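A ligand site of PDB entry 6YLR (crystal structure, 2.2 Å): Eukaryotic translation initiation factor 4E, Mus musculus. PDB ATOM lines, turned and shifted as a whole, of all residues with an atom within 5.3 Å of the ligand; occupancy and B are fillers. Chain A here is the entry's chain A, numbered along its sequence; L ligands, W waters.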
ATOM      1  N   PHE A  22      12.669  18.237  27.129  1.00  0.00           N
ATOM      2  CA  PHE A  22      11.674  17.209  27.361  1.00  0.00           C
ATOM      3  C   PHE A  22      11.743  16.172  26.247  1.00  0.00           C
ATOM      4  O   PHE A  22      11.659  16.524  25.063  1.00  0.00           O
ATOM      5  CB  PHE A  22      10.270  17.830  27.456  1.00  0.00           C
ATOM      6  CG  PHE A  22       9.174  16.831  27.731  1.00  0.00           C
ATOM      7  CD1 PHE A  22       8.660  16.040  26.716  1.00  0.00           C
ATOM      8  CD2 PHE A  22       8.684  16.668  29.007  1.00  0.00           C
ATOM      9  CE1 PHE A  22       7.658  15.124  26.974  1.00  0.00           C
ATOM     10  CE2 PHE A  22       7.695  15.763  29.275  1.00  0.00           C
ATOM     11  CZ  PHE A  22       7.180  14.980  28.254  1.00  0.00           C
ATOM     12  N   LYS A  23      11.887  14.910  26.627  1.00  0.00           N
ATOM     13  CA  LYS A  23      12.011  13.808  25.689  1.00  0.00           C
ATOM     14  C   LYS A  23      10.663  13.121  25.498  1.00  0.00           C
ATOM     15  O   LYS A  23       9.897  12.959  26.462  1.00  0.00           O
ATOM     16  CB  LYS A  23      13.041  12.797  26.194  1.00  0.00           C
ATOM     17  CG  LYS A  23      13.227  11.583  25.298  1.00  0.00           C
ATOM     18  CD  LYS A  23      14.085  11.907  24.097  1.00  0.00           C
ATOM     19  CE  LYS A  23      14.776  10.660  23.563  1.00  0.00           C
ATOM     20  NZ  LYS A  23      13.863   9.490  23.605  1.00  0.00           N
ATOM     21  N   ASP A  25       8.625  10.111  25.386  1.00  0.00           N
ATOM     22  CA  ASP A  25       8.699   8.714  25.825  1.00  0.00           C
ATOM     23  C   ASP A  25       7.442   8.434  26.653  1.00  0.00           C
ATOM     24  O   ASP A  25       7.332   8.886  27.787  1.00  0.00           O
ATOM     25  CB  ASP A  25       9.965   8.457  26.641  1.00  0.00           C
ATOM     26  CG  ASP A  25      10.173   6.980  26.954  1.00  0.00           C
ATOM     27  OD1 ASP A  25       9.288   6.159  26.637  1.00  0.00           O
ATOM     28  OD2 ASP A  25      11.236   6.641  27.513  1.00  0.00           O
ATOM     29  N   LYS A  26       6.510   7.682  26.065  1.00  0.00           N
ATOM     30  CA  LYS A  26       5.257   7.362  26.733  1.00  0.00           C
ATOM     31  C   LYS A  26       5.378   6.189  27.698  1.00  0.00           C
ATOM     32  O   LYS A  26       4.405   5.869  28.393  1.00  0.00           O
ATOM     33  CB  LYS A  26       4.168   7.062  25.699  1.00  0.00           C
ATOM     34  CG  LYS A  26       3.923   8.190  24.709  1.00  0.00           C
ATOM     35  CD  LYS A  26       3.843   9.533  25.404  1.00  0.00           C
ATOM     36  CE  LYS A  26       2.967  10.511  24.634  1.00  0.00           C
ATOM     37  NZ  LYS A  26       3.296  10.537  23.185  1.00  0.00           N
ATOM     38  N   SER A  27       6.543   5.556  27.771  1.00  0.00           N
ATOM     39  CA  SER A  27       6.781   4.523  28.766  1.00  0.00           C
ATOM     40  C   SER A  27       7.131   5.099  30.130  1.00  0.00           C
ATOM     41  O   SER A  27       7.081   4.370  31.130  1.00  0.00           O
ATOM     42  CB  SER A  27       7.896   3.582  28.310  1.00  0.00           C
ATOM     43  OG  SER A  27       9.138   4.254  28.223  1.00  0.00           O
ATOM     44  N   LYS A  28       7.481   6.387  30.202  1.00  0.00           N
ATOM     45  CA  LYS A  28       7.739   7.066  31.457  1.00  0.00           C
ATOM     46  C   LYS A  28       6.685   8.135  31.691  1.00  0.00           C
ATOM     47  O   LYS A  28       5.958   8.537  30.781  1.00  0.00           O
ATOM     48  CB  LYS A  28       9.139   7.713  31.447  1.00  0.00           C
ATOM     49  CG  LYS A  28      10.232   6.831  30.877  1.00  0.00           C
ATOM     50  CD  LYS A  28      11.511   7.624  30.628  1.00  0.00           C
ATOM     51  CE  LYS A  28      12.274   7.848  31.915  1.00  0.00           C
ATOM     52  NZ  LYS A  28      13.556   8.581  31.688  1.00  0.00           N
ATOM     53  N   THR A  29       6.583   8.580  32.941  1.00  0.00           N
ATOM     54  CA  THR A  29       5.648   9.651  33.274  1.00  0.00           C
ATOM     55  C   THR A  29       6.158  10.976  32.721  1.00  0.00           C
ATOM     56  O   THR A  29       7.303  11.110  32.299  1.00  0.00           O
ATOM     57  CB  THR A  29       5.449   9.740  34.783  1.00  0.00           C
ATOM     58  OG1 THR A  29       4.253  10.482  35.067  1.00  0.00           O
ATOM     59  CG2 THR A  29       6.640  10.414  35.452  1.00  0.00           C
ATOM     60  N   TRP A  30       5.272  11.989  32.738  1.00  0.00           N
ATOM     61  CA  TRP A  30       5.621  13.275  32.160  1.00  0.00           C
ATOM     62  C   TRP A  30       6.799  13.913  32.885  1.00  0.00           C
ATOM     63  O   TRP A  30       7.714  14.452  32.244  1.00  0.00           O
ATOM     64  CB  TRP A  30       4.415  14.222  32.173  1.00  0.00           C
ATOM     65  CG  TRP A  30       4.699  15.514  31.476  1.00  0.00           C
ATOM     66  CD1 TRP A  30       4.504  15.797  30.158  1.00  0.00           C
ATOM     67  CD2 TRP A  30       5.244  16.700  32.058  1.00  0.00           C
ATOM     68  NE1 TRP A  30       4.898  17.087  29.874  1.00  0.00           N
ATOM     69  CE2 TRP A  30       5.359  17.661  31.036  1.00  0.00           C
ATOM     70  CE3 TRP A  30       5.661  17.045  33.351  1.00  0.00           C
ATOM     71  CZ2 TRP A  30       5.854  18.945  31.258  1.00  0.00           C
ATOM     72  CZ3 TRP A  30       6.158  18.313  33.568  1.00  0.00           C
ATOM     73  CH2 TRP A  30       6.246  19.251  32.526  1.00  0.00           C
ATOM     74  N   GLN A  31       6.814  13.848  34.223  1.00  0.00           N
ATOM     75  CA  GLN A  31       7.896  14.466  34.977  1.00  0.00           C
ATOM     76  C   GLN A  31       9.232  13.801  34.703  1.00  0.00           C
ATOM     77  O   GLN A  31      10.279  14.455  34.673  1.00  0.00           O
ATOM     78  CB  GLN A  31       7.579  14.433  36.478  1.00  0.00           C
ATOM     79  CG  GLN A  31       6.347  15.215  36.882  1.00  0.00           C
ATOM     80  CD  GLN A  31       6.684  16.479  37.652  1.00  0.00           C
ATOM     81  OE1 GLN A  31       7.595  16.492  38.480  1.00  0.00           O
ATOM     82  NE2 GLN A  31       5.939  17.548  37.403  1.00  0.00           N
ATOM     83  N   ASN A  33      10.311  12.620  31.967  1.00  0.00           N
ATOM     84  CA  ASN A  33      10.815  12.956  30.642  1.00  0.00           C
ATOM     85  C   ASN A  33      11.465  14.341  30.570  1.00  0.00           C
ATOM     86  O   ASN A  33      12.004  14.697  29.514  1.00  0.00           O
ATOM     87  CB  ASN A  33       9.680  12.882  29.620  1.00  0.00           C
ATOM     88  CG  ASN A  33       9.295  11.445  29.301  1.00  0.00           C
ATOM     89  OD1 ASN A  33      10.142  10.570  29.206  1.00  0.00           O
ATOM     90  ND2 ASN A  33       7.988  11.209  29.135  1.00  0.00           N
ATOM     91  N   PRO A  74      10.052  24.376  34.598  1.00  0.00           N
ATOM     92  CA  PRO A  74       9.114  24.629  33.495  1.00  0.00           C
ATOM     93  C   PRO A  74       7.843  23.771  33.586  1.00  0.00           C
ATOM     94  O   PRO A  74       7.447  23.122  32.618  1.00  0.00           O
ATOM     95  CB  PRO A  74       9.940  24.282  32.256  1.00  0.00           C
ATOM     96  CG  PRO A  74      10.850  23.202  32.737  1.00  0.00           C
ATOM     97  CD  PRO A  74      11.182  23.540  34.168  1.00  0.00           C
ATOM     98  N   MET A  75       7.203  23.801  34.749  1.00  0.00           N
ATOM     99  CA  MET A  75       6.009  23.011  34.982  1.00  0.00           C
ATOM    100  C   MET A  75       4.973  23.855  35.715  1.00  0.00           C
ATOM    101  O   MET A  75       5.305  24.831  36.410  1.00  0.00           O
ATOM    102  CB  MET A  75       6.385  21.724  35.736  1.00  0.00           C
ATOM    103  CG  MET A  75       6.649  21.865  37.214  1.00  0.00           C
ATOM    104  SD  MET A  75       7.351  20.338  37.903  1.00  0.00           S
ATOM    105  CE  MET A  75       8.483  19.844  36.622  1.00  0.00           C
ATOM    106  N   TRP A  76       3.698  23.498  35.523  1.00  0.00           N
ATOM    107  CA  TRP A  76       2.602  24.320  36.022  1.00  0.00           C
ATOM    108  C   TRP A  76       2.424  24.218  37.534  1.00  0.00           C
ATOM    109  O   TRP A  76       1.710  25.059  38.107  1.00  0.00           O
ATOM    110  CB  TRP A  76       1.318  23.949  35.263  1.00  0.00           C
ATOM    111  CG  TRP A  76       0.756  22.559  35.482  1.00  0.00           C
ATOM    112  CD1 TRP A  76       0.750  21.835  36.636  1.00  0.00           C
ATOM    113  CD2 TRP A  76       0.096  21.752  34.498  1.00  0.00           C
ATOM    114  NE1 TRP A  76       0.130  20.625  36.437  1.00  0.00           N
ATOM    115  CE2 TRP A  76      -0.277  20.550  35.133  1.00  0.00           C
ATOM    116  CE3 TRP A  76      -0.215  21.932  33.146  1.00  0.00           C
ATOM    117  CZ2 TRP A  76      -0.944  19.525  34.457  1.00  0.00           C
ATOM    118  CZ3 TRP A  76      -0.875  20.913  32.475  1.00  0.00           C
ATOM    119  CH2 TRP A  76      -1.236  19.730  33.132  1.00  0.00           C
ATOM    120  N   GLU A  77       3.018  23.218  38.185  1.00  0.00           N
ATOM    121  CA  GLU A  77       2.927  23.083  39.638  1.00  0.00           C
ATOM    122  C   GLU A  77       4.032  23.836  40.374  1.00  0.00           C
ATOM    123  O   GLU A  77       4.054  23.819  41.609  1.00  0.00           O
ATOM    124  CB  GLU A  77       2.939  21.608  40.046  1.00  0.00           C
ATOM    125  CG  GLU A  77       4.109  20.798  39.496  1.00  0.00           C
ATOM    126  CD  GLU A  77       3.790  20.166  38.152  1.00  0.00           C
ATOM    127  OE1 GLU A  77       3.650  20.925  37.170  1.00  0.00           O
ATOM    128  OE2 GLU A  77       3.669  18.925  38.084  1.00  0.00           O
ATOM    129  N   ARG A  86       0.197  31.720  30.380  1.00  0.00           N
ATOM    130  CA  ARG A  86       1.084  31.770  29.223  1.00  0.00           C
ATOM    131  C   ARG A  86       0.401  32.449  28.051  1.00  0.00           C
ATOM    132  O   ARG A  86      -0.804  32.283  27.834  1.00  0.00           O
ATOM    133  CB  ARG A  86       1.549  30.358  28.828  1.00  0.00           C
ATOM    134  CG  ARG A  86       0.411  29.407  28.492  1.00  0.00           C
ATOM    135  CD  ARG A  86       0.918  28.021  28.135  1.00  0.00           C
ATOM    136  NE  ARG A  86      -0.188  27.106  27.835  1.00  0.00           N
ATOM    137  CZ  ARG A  86      -0.050  25.963  27.161  1.00  0.00           C
ATOM    138  NH1 ARG A  86      -1.109  25.197  26.934  1.00  0.00           N
ATOM    139  NH2 ARG A  86       1.139  25.589  26.703  1.00  0.00           N
ATOM    140  N   ARG A 131       5.250  19.319  17.972  1.00  0.00           N
ATOM    141  CA  ARG A 131       4.154  18.377  17.906  1.00  0.00           C
ATOM    142  C   ARG A 131       3.784  18.090  16.450  1.00  0.00           C
ATOM    143  O   ARG A 131       3.870  18.971  15.592  1.00  0.00           O
ATOM    144  CB  ARG A 131       2.902  18.896  18.645  1.00  0.00           C
ATOM    145  CG  ARG A 131       3.086  19.100  20.140  1.00  0.00           C
ATOM    146  CD  ARG A 131       3.712  17.881  20.789  1.00  0.00           C
ATOM    147  NE  ARG A 131       3.714  17.984  22.236  1.00  0.00           N
ATOM    148  CZ  ARG A 131       4.771  18.334  22.961  1.00  0.00           C
ATOM    149  NH1 ARG A 131       5.916  18.634  22.357  1.00  0.00           N
ATOM    150  NH2 ARG A 131       4.685  18.406  24.281  1.00  0.00           N
ATOM    151  N   LYS A 136       3.930  24.749  18.974  1.00  0.00           N
ATOM    152  CA  LYS A 136       3.453  25.801  19.856  1.00  0.00           C
ATOM    153  C   LYS A 136       4.623  26.441  20.569  1.00  0.00           C
ATOM    154  O   LYS A 136       5.595  25.767  20.922  1.00  0.00           O
ATOM    155  CB  LYS A 136       2.443  25.276  20.883  1.00  0.00           C
ATOM    156  CG  LYS A 136       1.149  24.749  20.288  1.00  0.00           C
ATOM    157  CD  LYS A 136       0.368  23.935  21.310  1.00  0.00           C
ATOM    158  CE  LYS A 136       1.059  22.626  21.617  1.00  0.00           C
ATOM    159  NZ  LYS A 136       0.373  21.874  22.705  1.00  0.00           N
ATOM    160  N   TRP A 140       5.637  32.300  29.595  1.00  0.00           N
ATOM    161  CA  TRP A 140       4.957  32.112  30.870  1.00  0.00           C
ATOM    162  C   TRP A 140       5.189  33.316  31.783  1.00  0.00           C
ATOM    163  O   TRP A 140       6.319  33.798  31.891  1.00  0.00           O
ATOM    164  CB  TRP A 140       5.450  30.844  31.570  1.00  0.00           C
ATOM    165  CG  TRP A 140       5.113  29.565  30.877  1.00  0.00           C
ATOM    166  CD1 TRP A 140       4.842  29.381  29.553  1.00  0.00           C
ATOM    167  CD2 TRP A 140       5.010  28.270  31.496  1.00  0.00           C
ATOM    168  NE1 TRP A 140       4.588  28.053  29.300  1.00  0.00           N
ATOM    169  CE2 TRP A 140       4.680  27.354  30.477  1.00  0.00           C
ATOM    170  CE3 TRP A 140       5.160  27.805  32.797  1.00  0.00           C
ATOM    171  CZ2 TRP A 140       4.501  26.000  30.728  1.00  0.00           C
ATOM    172  CZ3 TRP A 140       4.986  26.464  33.046  1.00  0.00           C
ATOM    173  CH2 TRP A 140       4.660  25.568  32.019  1.00  0.00           C
ATOM    174  N   HIS A 174      -2.686  28.783  33.848  1.00  0.00           N
ATOM    175  CA  HIS A 174      -2.154  27.431  34.014  1.00  0.00           C
ATOM    176  C   HIS A 174      -3.148  26.543  34.745  1.00  0.00           C
ATOM    177  O   HIS A 174      -3.380  25.397  34.343  1.00  0.00           O
ATOM    178  CB  HIS A 174      -0.821  27.470  34.757  1.00  0.00           C
ATOM    179  CG  HIS A 174       0.292  28.060  33.958  1.00  0.00           C
ATOM    180  ND1 HIS A 174       0.460  27.808  32.608  1.00  0.00           N
ATOM    181  CD2 HIS A 174       1.315  28.876  34.316  1.00  0.00           C
ATOM    182  CE1 HIS A 174       1.536  28.450  32.177  1.00  0.00           C
ATOM    183  NE2 HIS A 174       2.068  29.111  33.190  1.00  0.00           N
ATOM    184  N   THR A 177      -5.827  25.601  32.385  1.00  0.00           N
ATOM    185  CA  THR A 177      -5.341  24.641  31.391  1.00  0.00           C
ATOM    186  C   THR A 177      -5.137  23.256  32.003  1.00  0.00           C
ATOM    187  O   THR A 177      -5.460  22.245  31.374  1.00  0.00           O
ATOM    188  CB  THR A 177      -4.024  25.142  30.798  1.00  0.00           C
ATOM    189  OG1 THR A 177      -4.178  26.514  30.410  1.00  0.00           O
ATOM    190  CG2 THR A 177      -3.640  24.308  29.584  1.00  0.00           C
HETATM  191  C1  LIG L   1       2.279  21.973  30.404  1.00  0.00           C
HETATM  192  O1  LIG L   1       2.036  17.990  25.460  1.00  0.00           O
HETATM  193  C2  LIG L   1       2.493  23.103  31.185  1.00  0.00           C
HETATM  194  O2  LIG L   1       0.716  17.875  23.360  1.00  0.00           O
HETATM  195  C3  LIG L   1       1.601  24.172  31.127  1.00  0.00           C
HETATM  196  O3  LIG L   1       0.115  19.837  26.951  1.00  0.00           O
HETATM  197  O4  LIG L   1      -2.009  18.619  27.348  1.00  0.00           O
HETATM  198  C4  LIG L   1       1.264  16.378  31.359  1.00  0.00           C
HETATM  199  C5  LIG L   1      -0.016  11.668  27.064  1.00  0.00           C
HETATM  200  C6  LIG L   1       2.403  18.355  34.986  1.00  0.00           C
HETATM  201  C7  LIG L   1      -0.160  16.466  31.845  1.00  0.00           C
HETATM  202  C8  LIG L   1       3.109   9.700  29.291  1.00  0.00           C
HETATM  203  C9  LIG L   1      -1.088  12.716  27.307  1.00  0.00           C
HETATM  204  C10 LIG L   1      -0.852  16.780  30.569  1.00  0.00           C
HETATM  205  C11 LIG L   1      -2.163  12.187  26.406  1.00  0.00           C
HETATM  206  C12 LIG L   1       2.162  18.223  32.677  1.00  0.00           C
HETATM  207  C13 LIG L   1      -0.192  15.791  29.657  1.00  0.00           C
HETATM  208  C14 LIG L   1       2.205  11.458  28.042  1.00  0.00           C
HETATM  209  C15 LIG L   1      -1.395  11.740  25.155  1.00  0.00           C
HETATM  210  C16 LIG L   1       2.696  19.440  32.526  1.00  0.00           C
HETATM  211  C17 LIG L   1      -0.534  16.206  28.247  1.00  0.00           C
HETATM  212  C18 LIG L   1       3.345  12.154  28.120  1.00  0.00           C
HETATM  213  C19 LIG L   1      -1.564  12.787  24.035  1.00  0.00           C
HETATM  214  C20 LIG L   1       3.067  20.111  33.621  1.00  0.00           C
HETATM  215  C21 LIG L   1       4.387  11.658  28.780  1.00  0.00           C
HETATM  216  C22 LIG L   1       2.208  18.646  30.571  1.00  0.00           C
HETATM  217  C23 LIG L   1       1.926  13.315  26.972  1.00  0.00           C
HETATM  218  C24 LIG L   1       0.494  24.119  30.283  1.00  0.00           C
HETATM  219  C25 LIG L   1       0.287  22.986  29.496  1.00  0.00           C
HETATM  220  C26 LIG L   1       1.179  21.917  29.554  1.00  0.00           C
HETATM  221  C27 LIG L   1       3.197  20.916  30.454  1.00  0.00           C
HETATM  222  N1  LIG L   1       2.930  19.575  34.841  1.00  0.00           N
HETATM  223  N2  LIG L   1       4.300  10.402  29.395  1.00  0.00           N
HETATM  224  N3  LIG L   1       2.257  17.821  36.195  1.00  0.00           N
HETATM  225  N4  LIG L   1       2.975   8.504  29.863  1.00  0.00           N
HETATM  226  N5  LIG L   1       2.025  17.678  33.887  1.00  0.00           N
HETATM  227  N6  LIG L   1       2.080  10.251  28.615  1.00  0.00           N
HETATM  228  N7  LIG L   1       2.710  19.709  31.205  1.00  0.00           N
HETATM  229  N8  LIG L   1       3.167  13.296  27.462  1.00  0.00           N
HETATM  230  N9  LIG L   1       1.887  17.732  31.477  1.00  0.00           N
HETATM  231  N10 LIG L   1       1.333  12.188  27.339  1.00  0.00           N
HETATM  232  O5  LIG L   1      -0.552  15.157  32.246  1.00  0.00           O
HETATM  233  O6  LIG L   1      -1.521  12.638  28.672  1.00  0.00           O
HETATM  234  O7  LIG L   1      -2.251  16.456  30.681  1.00  0.00           O
HETATM  235  O8  LIG L   1      -2.805  11.049  27.008  1.00  0.00           O
HETATM  236  O9  LIG L   1       1.199  15.992  29.966  1.00  0.00           O
HETATM  237  O10 LIG L   1      -0.032  11.565  25.635  1.00  0.00           O
HETATM  238  O11 LIG L   1       0.103  17.445  27.956  1.00  0.00           O
HETATM  239  O12 LIG L   1      -1.301  14.193  24.252  1.00  0.00           O
HETATM  240  O13 LIG L   1       3.599  21.345  33.474  1.00  0.00           O
HETATM  241  O14 LIG L   1       5.442  12.296  28.855  1.00  0.00           O
HETATM  242  O15 LIG L   1       0.829  14.194  22.683  1.00  0.00           O
HETATM  243  O16 LIG L   1      -0.707  16.128  22.881  1.00  0.00           O
HETATM  244  O17 LIG L   1       0.871  15.760  24.735  1.00  0.00           O
HETATM  245  O18 LIG L   1      -0.550  17.774  25.507  1.00  0.00           O
HETATM  246  P1  LIG L   1      -0.037  14.994  23.637  1.00  0.00           P
HETATM  247  P2  LIG L   1       0.826  17.393  24.791  1.00  0.00           P
HETATM  248  P3  LIG L   1      -0.551  18.481  26.951  1.00  0.00           P
HETATM  249  O   HOH W   1       2.957  19.459  27.474  1.00  0.00           O
HETATM  250  O   HOH W   2      -3.634  15.480  25.865  1.00  0.00           O
HETATM  251  O   HOH W   3       7.096  11.764  26.475  1.00  0.00           O
HETATM  252  O   HOH W   4       3.983  16.018  26.366  1.00  0.00           O
HETATM  253  O   HOH W   5       5.701  22.124  28.522  1.00  0.00           O
HETATM  254  O   HOH W   6      -3.618  18.158  29.585  1.00  0.00           O
HETATM  255  O   HOH W   7       0.796  14.172  34.364  1.00  0.00           O
HETATM  256  O   HOH W   8      -0.439   8.351  26.852  1.00  0.00           O
HETATM  257  O   HOH W   9       0.277  16.772  20.709  1.00  0.00           O
HETATM  258  O   HOH W  10       0.417  12.441  30.757  1.00  0.00           O
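The side-chain carboxylate of Glu 77 lies within hydrogen-bond range of a nitrogen (N3) of the ligand, at 2.6 Å. The side-chain amide nitrogen of Asn 33 lies within hydrogen-bond range of an oxygen (O14) of the ligand (2.8 Å). A nitrogen (N2) of the ligand sits at hydrogen-bond distance from the backbone carbonyl oxygen (O) of Lys 28. The guanidinium group (NH2) of Arg 131 is in salt-bridge range of an oxygen (O1) of the ligand (2.9 Å). The backbone NH (N) of Trp 76 lies within hydrogen-bond range of an oxygen (O13) of the ligand (3.0 Å). A nitrogen (N1) of the ligand sits close to the indole nitrogen of Trp 76 (3.4 Å). A nitrogen (N4) of the ligand lies within hydrogen-bond range of the backbone carbonyl oxygen (O) of Lys 26, at 3.3 Å.
NE2 of Gln 31 lies within hydrogen-bond range of OE2 of Glu 77, 2.7 Å away. The side-chain amide nitrogen of Asn 33 sits at hydrogen-bond distance from the backbone carbonyl oxygen of Asp 25 (2.8 Å). The backbone carbonyl oxygen (O) of Thr 29 sits at hydrogen-bond distance from the side-chain amide nitrogen (ND2) of Asn 33. O of Asn 33 is in hydrogen-bond range of N of Lys 23, 2.9 Å away. The side-chain sulfur (SD) of Met 75 lies within hydrogen-bond range of the side-chain amide nitrogen (NE2) of Gln 31, at 3.2 Å. The side-chain hydroxyl (OG) of Ser 27 sits at hydrogen-bond distance from the side-chain carboxylate (OD1) of Asp 25 (2.5 Å).
NE1 of Trp 30 sits close to N9 of the ligand (3.5 Å). Merely in contact with the ligand: Phe 22 (3.3 Å), Met 75 (3.3 Å), Trp 140 (3.4 Å), Arg 86 (3.7 Å), Asp 25 (3.8 Å), Thr 29 (3.9 Å) and Gln 31 (3.9 Å). Hydrophobic or aromatic side chains that line the ligand: Phe 22, Trp 30, Met 75, Trp 76 and Trp 140. Along chain A the residues within 4 Å of the ligand span positions 22 to 140.
Water W4 bridges O1 of the ligand (2.9 Å) and NH2 of Arg 131 (3.2 Å). Water W3 lies within hydrogen-bond range of N of Asp 25 (2.5 Å), ND2 of Asn 33 (2.9 Å), O14 of the ligand (2.9 Å) and O of Lys 23 (3.0 Å).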
